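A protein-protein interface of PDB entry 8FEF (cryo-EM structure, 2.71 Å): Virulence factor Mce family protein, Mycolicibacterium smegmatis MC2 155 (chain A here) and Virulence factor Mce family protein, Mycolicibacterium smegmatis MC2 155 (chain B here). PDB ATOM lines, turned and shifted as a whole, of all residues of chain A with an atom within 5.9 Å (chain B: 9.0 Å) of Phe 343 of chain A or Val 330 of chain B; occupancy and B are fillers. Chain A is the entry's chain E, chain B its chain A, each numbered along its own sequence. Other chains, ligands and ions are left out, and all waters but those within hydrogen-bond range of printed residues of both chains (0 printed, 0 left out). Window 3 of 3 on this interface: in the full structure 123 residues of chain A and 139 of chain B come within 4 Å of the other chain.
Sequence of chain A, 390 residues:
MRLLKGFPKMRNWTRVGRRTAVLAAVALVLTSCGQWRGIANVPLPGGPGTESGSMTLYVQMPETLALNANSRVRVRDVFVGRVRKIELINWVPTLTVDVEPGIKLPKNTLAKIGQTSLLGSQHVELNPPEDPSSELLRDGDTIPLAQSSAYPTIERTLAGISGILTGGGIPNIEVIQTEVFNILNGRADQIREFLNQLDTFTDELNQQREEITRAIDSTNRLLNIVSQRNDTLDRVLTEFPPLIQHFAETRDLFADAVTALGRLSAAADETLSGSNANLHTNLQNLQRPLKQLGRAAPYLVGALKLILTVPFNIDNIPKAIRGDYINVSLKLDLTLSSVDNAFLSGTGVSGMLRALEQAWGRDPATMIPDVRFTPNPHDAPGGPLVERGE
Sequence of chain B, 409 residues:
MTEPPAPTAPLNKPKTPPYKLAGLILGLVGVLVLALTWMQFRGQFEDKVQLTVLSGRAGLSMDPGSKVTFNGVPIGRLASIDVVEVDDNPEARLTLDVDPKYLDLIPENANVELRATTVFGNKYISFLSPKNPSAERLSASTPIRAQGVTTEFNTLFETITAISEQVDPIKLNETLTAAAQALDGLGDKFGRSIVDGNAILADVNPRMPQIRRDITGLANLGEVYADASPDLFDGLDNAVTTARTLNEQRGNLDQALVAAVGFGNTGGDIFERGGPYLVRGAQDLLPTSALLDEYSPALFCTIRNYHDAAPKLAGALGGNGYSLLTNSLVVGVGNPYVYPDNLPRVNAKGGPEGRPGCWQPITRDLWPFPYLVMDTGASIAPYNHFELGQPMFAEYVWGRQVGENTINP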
ATOM      1  N   ASP A 333     -20.358  35.147   2.829  1.00  0.00           N
ATOM      2  CA  ASP A 333     -19.235  35.813   2.188  1.00  0.00           C
ATOM      3  C   ASP A 333     -19.487  35.863   0.687  1.00  0.00           C
ATOM      4  O   ASP A 333     -19.565  34.819   0.030  1.00  0.00           O
ATOM      5  CB  ASP A 333     -17.928  35.086   2.501  1.00  0.00           C
ATOM      6  CG  ASP A 333     -16.703  35.934   2.226  1.00  0.00           C
ATOM      7  OD1 ASP A 333     -16.802  36.900   1.444  1.00  0.00           O
ATOM      8  OD2 ASP A 333     -15.634  35.632   2.795  1.00  0.00           O
ATOM      9  N   LEU A 334     -19.617  37.076   0.149  1.00  0.00           N
ATOM     10  CA  LEU A 334     -19.782  37.293  -1.282  1.00  0.00           C
ATOM     11  C   LEU A 334     -18.668  38.172  -1.834  1.00  0.00           C
ATOM     12  O   LEU A 334     -18.811  38.752  -2.914  1.00  0.00           O
ATOM     13  CB  LEU A 334     -21.150  37.905  -1.580  1.00  0.00           C
ATOM     14  CG  LEU A 334     -22.349  37.116  -1.053  1.00  0.00           C
ATOM     15  CD1 LEU A 334     -23.655  37.813  -1.396  1.00  0.00           C
ATOM     16  CD2 LEU A 334     -22.338  35.700  -1.601  1.00  0.00           C
ATOM     17  N   SER A 338     -13.472  35.395  -2.002  1.00  0.00           N
ATOM     18  CA  SER A 338     -14.179  34.160  -1.686  1.00  0.00           C
ATOM     19  C   SER A 338     -14.845  33.576  -2.925  1.00  0.00           C
ATOM     20  O   SER A 338     -14.896  32.351  -3.088  1.00  0.00           O
ATOM     21  CB  SER A 338     -15.212  34.413  -0.591  1.00  0.00           C
ATOM     22  OG  SER A 338     -16.225  35.295  -1.042  1.00  0.00           O
ATOM     23  N   VAL A 339     -15.367  34.434  -3.804  1.00  0.00           N
ATOM     24  CA  VAL A 339     -15.956  33.962  -5.054  1.00  0.00           C
ATOM     25  C   VAL A 339     -14.891  33.319  -5.936  1.00  0.00           C
ATOM     26  O   VAL A 339     -15.145  32.312  -6.607  1.00  0.00           O
ATOM     27  CB  VAL A 339     -16.675  35.120  -5.770  1.00  0.00           C
ATOM     28  CG1 VAL A 339     -17.123  34.705  -7.160  1.00  0.00           C
ATOM     29  CG2 VAL A 339     -17.869  35.575  -4.953  1.00  0.00           C
ATOM     30  N   ASP A 340     -13.682  33.883  -5.943  1.00  0.00           N
ATOM     31  CA  ASP A 340     -12.588  33.281  -6.698  1.00  0.00           C
ATOM     32  C   ASP A 340     -12.220  31.914  -6.137  1.00  0.00           C
ATOM     33  O   ASP A 340     -12.108  30.934  -6.882  1.00  0.00           O
ATOM     34  CB  ASP A 340     -11.368  34.200  -6.678  1.00  0.00           C
ATOM     35  CG  ASP A 340     -10.118  33.526  -7.217  1.00  0.00           C
ATOM     36  OD1 ASP A 340     -10.228  32.664  -8.113  1.00  0.00           O
ATOM     37  OD2 ASP A 340      -9.017  33.845  -6.726  1.00  0.00           O
ATOM     38  N   ASN A 341     -12.014  31.832  -4.823  1.00  0.00           N
ATOM     39  CA  ASN A 341     -11.583  30.567  -4.236  1.00  0.00           C
ATOM     40  C   ASN A 341     -12.661  29.496  -4.343  1.00  0.00           C
ATOM     41  O   ASN A 341     -12.340  28.316  -4.521  1.00  0.00           O
ATOM     42  CB  ASN A 341     -11.175  30.765  -2.778  1.00  0.00           C
ATOM     43  CG  ASN A 341      -9.707  30.467  -2.543  1.00  0.00           C
ATOM     44  OD1 ASN A 341      -9.014  29.980  -3.433  1.00  0.00           O
ATOM     45  ND2 ASN A 341      -9.228  30.749  -1.340  1.00  0.00           N
ATOM     46  N   ALA A 342     -13.933  29.882  -4.241  1.00  0.00           N
ATOM     47  CA  ALA A 342     -15.010  28.899  -4.252  1.00  0.00           C
ATOM     48  C   ALA A 342     -15.192  28.274  -5.630  1.00  0.00           C
ATOM     49  O   ALA A 342     -15.280  27.049  -5.756  1.00  0.00           O
ATOM     50  CB  ALA A 342     -16.310  29.547  -3.783  1.00  0.00           C
ATOM     51  N   PHE A 343     -15.245  29.097  -6.678  1.00  0.00           N
ATOM     52  CA  PHE A 343     -15.612  28.624  -8.008  1.00  0.00           C
ATOM     53  C   PHE A 343     -14.427  28.541  -8.962  1.00  0.00           C
ATOM     54  O   PHE A 343     -14.165  27.481  -9.537  1.00  0.00           O
ATOM     55  CB  PHE A 343     -16.696  29.529  -8.608  1.00  0.00           C
ATOM     56  CG  PHE A 343     -17.933  29.639  -7.769  1.00  0.00           C
ATOM     57  CD1 PHE A 343     -18.661  28.511  -7.434  1.00  0.00           C
ATOM     58  CD2 PHE A 343     -18.379  30.872  -7.331  1.00  0.00           C
ATOM     59  CE1 PHE A 343     -19.804  28.611  -6.667  1.00  0.00           C
ATOM     60  CE2 PHE A 343     -19.523  30.979  -6.565  1.00  0.00           C
ATOM     61  CZ  PHE A 343     -20.236  29.846  -6.234  1.00  0.00           C
ATOM     62  N   LEU A 344     -13.700  29.640  -9.148  1.00  0.00           N
ATOM     63  CA  LEU A 344     -12.758  29.773 -10.250  1.00  0.00           C
ATOM     64  C   LEU A 344     -11.370  29.233  -9.928  1.00  0.00           C
ATOM     65  O   LEU A 344     -10.408  29.584 -10.619  1.00  0.00           O
ATOM     66  CB  LEU A 344     -12.668  31.237 -10.685  1.00  0.00           C
ATOM     67  CG  LEU A 344     -14.004  31.963 -10.873  1.00  0.00           C
ATOM     68  CD1 LEU A 344     -13.772  33.356 -11.412  1.00  0.00           C
ATOM     69  CD2 LEU A 344     -14.940  31.189 -11.790  1.00  0.00           C
ATOM     70  N   SER A 345     -11.239  28.401  -8.900  1.00  0.00           N
ATOM     71  CA  SER A 345      -9.970  27.738  -8.633  1.00  0.00           C
ATOM     72  C   SER A 345      -9.806  26.545  -9.562  1.00  0.00           C
ATOM     73  O   SER A 345     -10.763  25.818  -9.841  1.00  0.00           O
ATOM     74  CB  SER A 345      -9.890  27.283  -7.176  1.00  0.00           C
ATOM     75  OG  SER A 345      -9.778  28.389  -6.300  1.00  0.00           O
ATOM     76  N   GLY A 346      -8.585  26.347 -10.049  1.00  0.00           N
ATOM     77  CA  GLY A 346      -8.322  25.262 -10.967  1.00  0.00           C
ATOM     78  C   GLY A 346      -8.783  25.497 -12.385  1.00  0.00           C
ATOM     79  O   GLY A 346      -8.816  24.546 -13.174  1.00  0.00           O
ATOM     80  N   THR A 347      -9.147  26.724 -12.736  1.00  0.00           N
ATOM     81  CA  THR A 347      -9.558  27.079 -14.086  1.00  0.00           C
ATOM     82  C   THR A 347      -8.612  28.142 -14.639  1.00  0.00           C
ATOM     83  O   THR A 347      -7.610  28.501 -14.014  1.00  0.00           O
ATOM     84  CB  THR A 347     -11.010  27.562 -14.101  1.00  0.00           C
ATOM     85  OG1 THR A 347     -11.150  28.692 -13.233  1.00  0.00           O
ATOM     86  CG2 THR A 347     -11.947  26.458 -13.644  1.00  0.00           C
ATOM     87  N   ASN B 327     -17.713  31.581   8.874  1.00  0.00           N
ATOM     88  CA  ASN B 327     -17.620  32.295   7.606  1.00  0.00           C
ATOM     89  C   ASN B 327     -18.170  31.397   6.505  1.00  0.00           C
ATOM     90  O   ASN B 327     -17.625  30.318   6.250  1.00  0.00           O
ATOM     91  CB  ASN B 327     -16.175  32.688   7.302  1.00  0.00           C
ATOM     92  CG  ASN B 327     -15.993  34.183   7.167  1.00  0.00           C
ATOM     93  OD1 ASN B 327     -16.941  34.911   6.873  1.00  0.00           O
ATOM     94  ND2 ASN B 327     -14.769  34.652   7.373  1.00  0.00           N
ATOM     95  N   SER B 328     -19.235  31.844   5.848  1.00  0.00           N
ATOM     96  CA  SER B 328     -19.965  31.025   4.892  1.00  0.00           C
ATOM     97  C   SER B 328     -19.836  31.610   3.493  1.00  0.00           C
ATOM     98  O   SER B 328     -20.121  32.791   3.280  1.00  0.00           O
ATOM     99  CB  SER B 328     -21.437  30.911   5.283  1.00  0.00           C
ATOM    100  OG  SER B 328     -21.575  30.296   6.551  1.00  0.00           O
ATOM    101  N   LEU B 329     -19.402  30.781   2.549  1.00  0.00           N
ATOM    102  CA  LEU B 329     -19.394  31.121   1.134  1.00  0.00           C
ATOM    103  C   LEU B 329     -19.941  29.944   0.344  1.00  0.00           C
ATOM    104  O   LEU B 329     -19.617  28.790   0.637  1.00  0.00           O
ATOM    105  CB  LEU B 329     -17.979  31.488   0.663  1.00  0.00           C
ATOM    106  CG  LEU B 329     -16.833  30.538   1.030  1.00  0.00           C
ATOM    107  CD1 LEU B 329     -16.548  29.539  -0.078  1.00  0.00           C
ATOM    108  CD2 LEU B 329     -15.578  31.316   1.387  1.00  0.00           C
ATOM    109  N   VAL B 330     -20.790  30.234  -0.645  1.00  0.00           N
ATOM    110  CA  VAL B 330     -21.394  29.168  -1.431  1.00  0.00           C
ATOM    111  C   VAL B 330     -20.332  28.501  -2.301  1.00  0.00           C
ATOM    112  O   VAL B 330     -19.384  29.142  -2.770  1.00  0.00           O
ATOM    113  CB  VAL B 330     -22.563  29.704  -2.279  1.00  0.00           C
ATOM    114  CG1 VAL B 330     -23.678  30.208  -1.376  1.00  0.00           C
ATOM    115  CG2 VAL B 330     -22.092  30.811  -3.204  1.00  0.00           C
ATOM    116  N   VAL B 331     -20.483  27.193  -2.503  1.00  0.00           N
ATOM    117  CA  VAL B 331     -19.498  26.382  -3.208  1.00  0.00           C
ATOM    118  C   VAL B 331     -20.230  25.226  -3.883  1.00  0.00           C
ATOM    119  O   VAL B 331     -21.413  24.983  -3.633  1.00  0.00           O
ATOM    120  CB  VAL B 331     -18.400  25.866  -2.246  1.00  0.00           C
ATOM    121  CG1 VAL B 331     -18.900  24.669  -1.451  1.00  0.00           C
ATOM    122  CG2 VAL B 331     -17.102  25.552  -2.986  1.00  0.00           C
ATOM    123  N   GLY B 332     -19.529  24.517  -4.765  1.00  0.00           N
ATOM    124  CA  GLY B 332     -20.074  23.326  -5.394  1.00  0.00           C
ATOM    125  C   GLY B 332     -19.700  22.063  -4.633  1.00  0.00           C
ATOM    126  O   GLY B 332     -18.606  21.954  -4.081  1.00  0.00           O
ATOM    127  N   VAL B 333     -20.625  21.109  -4.614  1.00  0.00           N
ATOM    128  CA  VAL B 333     -20.460  19.855  -3.885  1.00  0.00           C
ATOM    129  C   VAL B 333     -20.055  18.754  -4.849  1.00  0.00           C
ATOM    130  O   VAL B 333     -20.485  18.729  -6.009  1.00  0.00           O
ATOM    131  CB  VAL B 333     -21.734  19.465  -3.112  1.00  0.00           C
ATOM    132  CG1 VAL B 333     -22.020  20.471  -2.048  1.00  0.00           C
ATOM    133  CG2 VAL B 333     -22.913  19.392  -4.050  1.00  0.00           C
ATOM    134  N   ASN B 384     -10.096  18.394  -9.166  1.00  0.00           N
ATOM    135  CA  ASN B 384      -9.112  19.408  -9.512  1.00  0.00           C
ATOM    136  C   ASN B 384      -9.656  20.474 -10.450  1.00  0.00           C
ATOM    137  O   ASN B 384      -8.939  21.430 -10.759  1.00  0.00           O
ATOM    138  CB  ASN B 384      -7.889  18.753 -10.161  1.00  0.00           C
ATOM    139  CG  ASN B 384      -7.321  17.627  -9.331  1.00  0.00           C
ATOM    140  OD1 ASN B 384      -7.403  17.642  -8.105  1.00  0.00           O
ATOM    141  ND2 ASN B 384      -6.741  16.637  -9.997  1.00  0.00           N
ATOM    142  N   HIS B 385     -10.894  20.336 -10.912  1.00  0.00           N
ATOM    143  CA  HIS B 385     -11.394  21.171 -11.992  1.00  0.00           C
ATOM    144  C   HIS B 385     -12.897  21.359 -11.830  1.00  0.00           C
ATOM    145  O   HIS B 385     -13.552  20.668 -11.046  1.00  0.00           O
ATOM    146  CB  HIS B 385     -10.966  20.587 -13.345  1.00  0.00           C
ATOM    147  CG  HIS B 385     -11.457  19.198 -13.594  1.00  0.00           C
ATOM    148  ND1 HIS B 385     -10.911  18.095 -12.973  1.00  0.00           N
ATOM    149  CD2 HIS B 385     -12.385  18.721 -14.452  1.00  0.00           C
ATOM    150  CE1 HIS B 385     -11.521  17.004 -13.398  1.00  0.00           C
ATOM    151  NE2 HIS B 385     -12.420  17.357 -14.297  1.00  0.00           N
ATOM    152  N   PHE B 386     -13.438  22.309 -12.589  1.00  0.00           N
ATOM    153  CA  PHE B 386     -14.875  22.564 -12.629  1.00  0.00           C
ATOM    154  C   PHE B 386     -15.587  21.642 -13.612  1.00  0.00           C
ATOM    155  O   PHE B 386     -15.321  21.685 -14.819  1.00  0.00           O
ATOM    156  CB  PHE B 386     -15.127  24.027 -12.995  1.00  0.00           C
ATOM    157  CG  PHE B 386     -16.571  24.351 -13.273  1.00  0.00           C
ATOM    158  CD1 PHE B 386     -17.416  24.711 -12.240  1.00  0.00           C
ATOM    159  CD2 PHE B 386     -17.077  24.321 -14.564  1.00  0.00           C
ATOM    160  CE1 PHE B 386     -18.737  25.020 -12.486  1.00  0.00           C
ATOM    161  CE2 PHE B 386     -18.400  24.621 -14.812  1.00  0.00           C
ATOM    162  CZ  PHE B 386     -19.231  24.971 -13.772  1.00  0.00           C
ATOM    163  N   GLU B 387     -16.488  20.806 -13.096  1.00  0.00           N
ATOM    164  CA  GLU B 387     -17.303  19.926 -13.922  1.00  0.00           C
ATOM    165  C   GLU B 387     -18.736  19.908 -13.427  1.00  0.00           C
ATOM    166  O   GLU B 387     -19.010  20.125 -12.245  1.00  0.00           O
ATOM    167  CB  GLU B 387     -16.792  18.490 -13.954  1.00  0.00           C
ATOM    168  CG  GLU B 387     -15.564  18.318 -14.771  1.00  0.00           C
ATOM    169  CD  GLU B 387     -15.420  16.924 -15.318  1.00  0.00           C
ATOM    170  OE1 GLU B 387     -16.405  16.160 -15.276  1.00  0.00           O
ATOM    171  OE2 GLU B 387     -14.313  16.587 -15.777  1.00  0.00           O
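N of Asp 333 of chain A lies within hydrogen-bond range of O of Ser 328 of chain B, 2.4 Å away.
The side-chain carboxylate (OD1) of Asp 333 of chain A lies within hydrogen-bond range of the side-chain hydroxyl (OG) of Ser 338 of chain A (3.0 Å).
Among the printed residues, merely in contact across the chains: Ala 342 of chain A with Val 330 of chain B (3.3 Å), Phe 343 of chain A with Val 330 of chain B (3.6 Å), Ala 342 of chain A with Val 331 of chain B (3.6 Å), Ser 338 of chain A with Leu 329 of chain B (3.7 Å), Ala 342 of chain A with Leu 329 of chain B (3.7 Å), Asp 333 of chain A with Leu 329 of chain B (3.7 Å) and Gly 346 of chain A with Asn 384 of chain B (3.9 Å).
Printed residues of chain B within 4 Å of Asp 333 of chain A: Ser 328 (2.4 Å) and Leu 329 (3.7 Å). Of the printed residues of chain B, Ser 338 of chain A touches Leu 329. Ala 342 of chain A touches three residues of chain B. Phe 343 of chain A touches just one residue of chain B: Val 330 (3.6 Å). Of the printed residues of chain B, Gly 346 of chain A touches Asn 384 (3.9 Å). Of the printed residues of chain A, Ser 328 of chain B touches Asp 333. Of the printed residues of chain A, Leu 329 of chain B touches Asp 333 (3.7 Å), Ser 338 (3.7 Å) and Ala 342 (3.7 Å). Printed residues of chain A within 4 Å of Val 330 of chain B: Ala 342 and Phe 343. The nearest printed residue of chain A that does not touch Asn 384 of chain B is Ser 345 of chain A (4.8 Å).
Hydrophobic or aromatic side chains of chain A that line the printed part of chain B: Ala 342 and Phe 343. Hydrophobic or aromatic side chains of chain B that line the printed part of chain A: Leu 329, Val 330 and Val 331. Among the printed residues, 8 pairs touch across the chains. Among the printed residues, no Asp or Glu carboxylate lies within 4 Å of a Lys or Arg side-chain nitrogen of the other chain.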
